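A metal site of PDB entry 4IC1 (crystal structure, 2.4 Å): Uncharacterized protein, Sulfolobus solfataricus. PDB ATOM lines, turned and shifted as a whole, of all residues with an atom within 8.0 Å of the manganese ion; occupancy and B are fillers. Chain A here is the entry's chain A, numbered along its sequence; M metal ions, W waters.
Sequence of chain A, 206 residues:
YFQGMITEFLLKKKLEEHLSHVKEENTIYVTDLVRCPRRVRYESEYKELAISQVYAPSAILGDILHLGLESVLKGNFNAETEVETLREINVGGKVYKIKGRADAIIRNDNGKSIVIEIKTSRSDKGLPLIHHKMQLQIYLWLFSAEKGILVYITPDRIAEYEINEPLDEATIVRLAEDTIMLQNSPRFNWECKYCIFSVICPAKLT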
ATOM      1  N   THR A  31      20.602  34.340  24.724  1.00  0.00           N
ATOM      2  CA  THR A  31      21.217  33.165  25.382  1.00  0.00           C
ATOM      3  C   THR A  31      21.291  33.361  26.902  1.00  0.00           C
ATOM      4  O   THR A  31      21.097  32.443  27.636  1.00  0.00           O
ATOM      5  CB  THR A  31      22.618  32.768  24.784  1.00  0.00           C
ATOM      6  OG1 THR A  31      23.419  33.926  24.611  1.00  0.00           O
ATOM      7  CG2 THR A  31      22.477  32.191  23.426  1.00  0.00           C
ATOM      8  N   GLY A  62      31.546  23.062  17.493  1.00  0.00           N
ATOM      9  CA  GLY A  62      30.257  23.732  17.295  1.00  0.00           C
ATOM     10  C   GLY A  62      30.364  24.864  16.341  1.00  0.00           C
ATOM     11  O   GLY A  62      29.505  24.993  15.502  1.00  0.00           O
ATOM     12  N   ASP A  63      31.418  25.683  16.432  1.00  0.00           N
ATOM     13  CA  ASP A  63      31.431  26.881  15.618  1.00  0.00           C
ATOM     14  C   ASP A  63      31.690  26.544  14.190  1.00  0.00           C
ATOM     15  O   ASP A  63      31.115  27.162  13.344  1.00  0.00           O
ATOM     16  CB  ASP A  63      32.513  27.873  16.047  1.00  0.00           C
ATOM     17  CG  ASP A  63      32.254  28.522  17.391  1.00  0.00           C
ATOM     18  OD1 ASP A  63      31.071  28.560  17.843  1.00  0.00           O
ATOM     19  OD2 ASP A  63      33.265  29.002  17.999  1.00  0.00           O
ATOM     20  N   HIS A  66      28.468  25.164  12.654  1.00  0.00           N
ATOM     21  CA  HIS A  66      27.640  26.284  12.293  1.00  0.00           C
ATOM     22  C   HIS A  66      28.168  26.835  10.986  1.00  0.00           C
ATOM     23  O   HIS A  66      27.439  26.984  10.046  1.00  0.00           O
ATOM     24  CB  HIS A  66      27.613  27.363  13.362  1.00  0.00           C
ATOM     25  CG  HIS A  66      26.675  27.055  14.493  1.00  0.00           C
ATOM     26  ND1 HIS A  66      26.989  26.174  15.506  1.00  0.00           N
ATOM     27  CD2 HIS A  66      25.458  27.566  14.799  1.00  0.00           C
ATOM     28  CE1 HIS A  66      25.999  26.140  16.393  1.00  0.00           C
ATOM     29  NE2 HIS A  66      25.053  26.987  15.986  1.00  0.00           N
ATOM     30  N   GLU A  70      25.636  26.769   8.092  1.00  0.00           N
ATOM     31  CA  GLU A  70      25.387  28.134   7.593  1.00  0.00           C
ATOM     32  C   GLU A  70      25.752  28.312   6.113  1.00  0.00           C
ATOM     33  O   GLU A  70      24.911  28.816   5.396  1.00  0.00           O
ATOM     34  CB  GLU A  70      26.021  29.213   8.442  1.00  0.00           C
ATOM     35  CG  GLU A  70      25.195  29.443   9.675  1.00  0.00           C
ATOM     36  CD  GLU A  70      25.947  30.198  10.742  1.00  0.00           C
ATOM     37  OE1 GLU A  70      27.022  30.791  10.436  1.00  0.00           O
ATOM     38  OE2 GLU A  70      25.485  30.173  11.884  1.00  0.00           O
ATOM     39  N   ARG A 101      21.193  36.916  18.046  1.00  0.00           N
ATOM     40  CA  ARG A 101      21.782  36.653  16.811  1.00  0.00           C
ATOM     41  C   ARG A 101      21.431  35.243  16.360  1.00  0.00           C
ATOM     42  O   ARG A 101      21.818  34.237  16.991  1.00  0.00           O
ATOM     43  CB  ARG A 101      23.280  36.806  16.851  1.00  0.00           C
ATOM     44  CG  ARG A 101      23.834  36.860  15.453  1.00  0.00           C
ATOM     45  CD  ARG A 101      25.048  35.999  15.309  1.00  0.00           C
ATOM     46  NE  ARG A 101      26.245  36.515  15.924  1.00  0.00           N
ATOM     47  CZ  ARG A 101      27.379  35.817  15.979  1.00  0.00           C
ATOM     48  NH1 ARG A 101      27.400  34.563  15.465  1.00  0.00           N
ATOM     49  NH2 ARG A 101      28.489  36.318  16.540  1.00  0.00           N
ATOM     50  N   ALA A 102      20.685  35.200  15.258  1.00  0.00           N
ATOM     51  CA  ALA A 102      20.134  33.998  14.742  1.00  0.00           C
ATOM     52  C   ALA A 102      21.185  33.329  13.896  1.00  0.00           C
ATOM     53  O   ALA A 102      21.892  33.964  13.147  1.00  0.00           O
ATOM     54  CB  ALA A 102      18.901  34.365  13.905  1.00  0.00           C
ATOM     55  N   ASP A 103      21.270  32.025  13.925  1.00  0.00           N
ATOM     56  CA  ASP A 103      22.280  31.361  13.112  1.00  0.00           C
ATOM     57  C   ASP A 103      21.966  31.582  11.649  1.00  0.00           C
ATOM     58  O   ASP A 103      22.867  31.815  10.868  1.00  0.00           O
ATOM     59  CB  ASP A 103      22.283  29.849  13.394  1.00  0.00           C
ATOM     60  CG  ASP A 103      22.736  29.507  14.787  1.00  0.00           C
ATOM     61  OD1 ASP A 103      23.355  30.387  15.427  1.00  0.00           O
ATOM     62  OD2 ASP A 103      22.471  28.343  15.218  1.00  0.00           O
ATOM     63  N   ALA A 104      20.688  31.423  11.285  1.00  0.00           N
ATOM     64  CA  ALA A 104      20.209  31.756   9.916  1.00  0.00           C
ATOM     65  C   ALA A 104      18.749  32.158   9.929  1.00  0.00           C
ATOM     66  O   ALA A 104      17.978  31.733  10.800  1.00  0.00           O
ATOM     67  CB  ALA A 104      20.450  30.617   8.926  1.00  0.00           C
ATOM     68  N   ILE A 116      16.297  29.914  11.996  1.00  0.00           N
ATOM     69  CA  ILE A 116      16.936  28.612  12.154  1.00  0.00           C
ATOM     70  C   ILE A 116      18.001  28.634  13.260  1.00  0.00           C
ATOM     71  O   ILE A 116      18.820  29.510  13.309  1.00  0.00           O
ATOM     72  CB  ILE A 116      17.539  28.209  10.840  1.00  0.00           C
ATOM     73  CG1 ILE A 116      16.377  28.117   9.826  1.00  0.00           C
ATOM     74  CG2 ILE A 116      18.276  26.901  10.947  1.00  0.00           C
ATOM     75  CD1 ILE A 116      16.829  28.058   8.415  1.00  0.00           C
ATOM     76  N   GLU A 117      17.915  27.698  14.188  1.00  0.00           N
ATOM     77  CA  GLU A 117      18.857  27.583  15.249  1.00  0.00           C
ATOM     78  C   GLU A 117      19.482  26.241  15.140  1.00  0.00           C
ATOM     79  O   GLU A 117      18.768  25.251  15.142  1.00  0.00           O
ATOM     80  CB  GLU A 117      18.146  27.745  16.551  1.00  0.00           C
ATOM     81  CG  GLU A 117      19.092  27.598  17.801  1.00  0.00           C
ATOM     82  CD  GLU A 117      20.252  28.615  17.858  1.00  0.00           C
ATOM     83  OE1 GLU A 117      21.374  28.219  18.273  1.00  0.00           O
ATOM     84  OE2 GLU A 117      20.022  29.789  17.541  1.00  0.00           O
ATOM     85  N   ILE A 118      20.809  26.193  15.002  1.00  0.00           N
ATOM     86  CA  ILE A 118      21.528  24.945  14.791  1.00  0.00           C
ATOM     87  C   ILE A 118      22.148  24.502  16.109  1.00  0.00           C
ATOM     88  O   ILE A 118      22.654  25.328  16.833  1.00  0.00           O
ATOM     89  CB  ILE A 118      22.631  25.050  13.746  1.00  0.00           C
ATOM     90  CG1 ILE A 118      22.115  25.679  12.434  1.00  0.00           C
ATOM     91  CG2 ILE A 118      23.156  23.664  13.434  1.00  0.00           C
ATOM     92  CD1 ILE A 118      23.224  26.247  11.455  1.00  0.00           C
ATOM     93  N   LYS A 119      22.095  23.215  16.446  1.00  0.00           N
ATOM     94  CA  LYS A 119      22.716  22.722  17.709  1.00  0.00           C
ATOM     95  C   LYS A 119      23.497  21.518  17.401  1.00  0.00           C
ATOM     96  O   LYS A 119      23.159  20.778  16.488  1.00  0.00           O
ATOM     97  CB  LYS A 119      21.680  22.371  18.737  1.00  0.00           C
ATOM     98  CG  LYS A 119      20.871  23.556  19.250  1.00  0.00           C
ATOM     99  CD  LYS A 119      21.789  24.616  19.943  1.00  0.00           C
ATOM    100  CE  LYS A 119      20.947  25.698  20.549  1.00  0.00           C
ATOM    101  NZ  LYS A 119      21.667  26.997  20.796  1.00  0.00           N
ATOM    102  N   THR A 120      24.586  21.325  18.129  1.00  0.00           N
ATOM    103  CA  THR A 120      25.396  20.116  17.952  1.00  0.00           C
ATOM    104  C   THR A 120      25.650  19.601  19.343  1.00  0.00           C
ATOM    105  O   THR A 120      26.049  20.358  20.154  1.00  0.00           O
ATOM    106  CB  THR A 120      26.704  20.484  17.242  1.00  0.00           C
ATOM    107  OG1 THR A 120      27.527  21.266  18.132  1.00  0.00           O
ATOM    108  CG2 THR A 120      26.423  21.388  15.996  1.00  0.00           C
ATOM    109  N   HIS A 132      17.060  24.871  24.604  1.00  0.00           N
ATOM    110  CA  HIS A 132      17.223  25.153  23.196  1.00  0.00           C
ATOM    111  C   HIS A 132      15.894  25.592  22.565  1.00  0.00           C
ATOM    112  O   HIS A 132      15.823  26.597  21.889  1.00  0.00           O
ATOM    113  CB  HIS A 132      17.723  23.932  22.523  1.00  0.00           C
ATOM    114  CG  HIS A 132      19.090  23.551  22.919  1.00  0.00           C
ATOM    115  ND1 HIS A 132      19.603  22.301  22.662  1.00  0.00           N
ATOM    116  CD2 HIS A 132      20.065  24.259  23.545  1.00  0.00           C
ATOM    117  CE1 HIS A 132      20.854  22.281  23.091  1.00  0.00           C
ATOM    118  NE2 HIS A 132      21.163  23.461  23.619  1.00  0.00           N
ATOM    119  N   GLN A 135      15.241  29.322  23.690  1.00  0.00           N
ATOM    120  CA  GLN A 135      16.062  30.201  22.926  1.00  0.00           C
ATOM    121  C   GLN A 135      15.367  30.525  21.627  1.00  0.00           C
ATOM    122  O   GLN A 135      15.159  31.656  21.302  1.00  0.00           O
ATOM    123  CB  GLN A 135      17.408  29.530  22.639  1.00  0.00           C
ATOM    124  CG  GLN A 135      18.418  30.445  21.939  1.00  0.00           C
ATOM    125  CD  GLN A 135      19.780  29.776  21.728  1.00  0.00           C
ATOM    126  OE1 GLN A 135      20.033  28.637  22.193  1.00  0.00           O
ATOM    127  NE2 GLN A 135      20.663  30.471  21.031  1.00  0.00           N
ATOM    128  N   TYR A 139      13.927  33.980  19.965  1.00  0.00           N
ATOM    129  CA  TYR A 139      14.251  34.543  18.671  1.00  0.00           C
ATOM    130  C   TYR A 139      12.959  34.838  17.817  1.00  0.00           C
ATOM    131  O   TYR A 139      12.810  35.909  17.275  1.00  0.00           O
ATOM    132  CB  TYR A 139      15.200  33.625  17.921  1.00  0.00           C
ATOM    133  CG  TYR A 139      16.574  33.520  18.497  1.00  0.00           C
ATOM    134  CD1 TYR A 139      17.199  34.607  19.078  1.00  0.00           C
ATOM    135  CD2 TYR A 139      17.311  32.394  18.367  1.00  0.00           C
ATOM    136  CE1 TYR A 139      18.458  34.495  19.609  1.00  0.00           C
ATOM    137  CE2 TYR A 139      18.586  32.295  18.893  1.00  0.00           C
ATOM    138  CZ  TYR A 139      19.149  33.335  19.491  1.00  0.00           C
ATOM    139  OH  TYR A 139      20.442  33.232  19.986  1.00  0.00           O
ATOM    140  N   LEU A 150      14.674  24.188  14.639  1.00  0.00           N
ATOM    141  CA  LEU A 150      15.745  23.765  15.540  1.00  0.00           C
ATOM    142  C   LEU A 150      16.336  22.477  14.996  1.00  0.00           C
ATOM    143  O   LEU A 150      15.685  21.460  15.065  1.00  0.00           O
ATOM    144  CB  LEU A 150      15.149  23.557  16.931  1.00  0.00           C
ATOM    145  CG  LEU A 150      16.048  23.026  18.025  1.00  0.00           C
ATOM    146  CD1 LEU A 150      17.218  23.951  18.285  1.00  0.00           C
ATOM    147  CD2 LEU A 150      15.272  22.845  19.312  1.00  0.00           C
ATOM    148  N   VAL A 151      17.537  22.511  14.430  1.00  0.00           N
ATOM    149  CA  VAL A 151      18.116  21.294  13.844  1.00  0.00           C
ATOM    150  C   VAL A 151      19.337  20.854  14.643  1.00  0.00           C
ATOM    151  O   VAL A 151      20.202  21.677  14.902  1.00  0.00           O
ATOM    152  CB  VAL A 151      18.510  21.477  12.373  1.00  0.00           C
ATOM    153  CG1 VAL A 151      19.257  22.741  12.179  1.00  0.00           C
ATOM    154  CG2 VAL A 151      19.325  20.343  11.902  1.00  0.00           C
HETATM  155 MN    MN M   1      23.232  27.548  17.316  1.00  0.00          MN
HETATM  156  O   HOH W   1      24.161  29.950  17.760  1.00  0.00           O
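The side-chain carboxylate (OE1) of Glu 117 sits close to the side-chain amino group (NZ) of Lys 119, 2.8 Å away. O of Glu 117 is in hydrogen-bond range of N of Val 151, at 3.1 Å. O of Gly 62 sits at hydrogen-bond distance from ND1 of His 66 (2.8 Å). The side-chain amino group of Lys 119 lies within hydrogen-bond range of the side-chain amide oxygen of Gln 135 (2.7 Å). N of Lys 119 sits at hydrogen-bond distance from O of Val 151 (2.9 Å).
The manganese ion is bound by the side-chain carboxylate (OE1) of Glu 117 (2.2 Å), a ring nitrogen (NE2) of His 66 (2.3 Å), the backbone carbonyl oxygen (O) of Ile 118 (2.3 Å), the side-chain carboxylate (OD2) of Asp 103 (2.4 Å) and water W1 (2.6 Å).
Lys 119 touches the manganese ion. Within 4 Å of the manganese ion: His 66, Asp 103, Glu 117, Ile 118 and Lys 119. Along chain A the residues within 4 Å of the manganese ion span positions 66 to 119.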
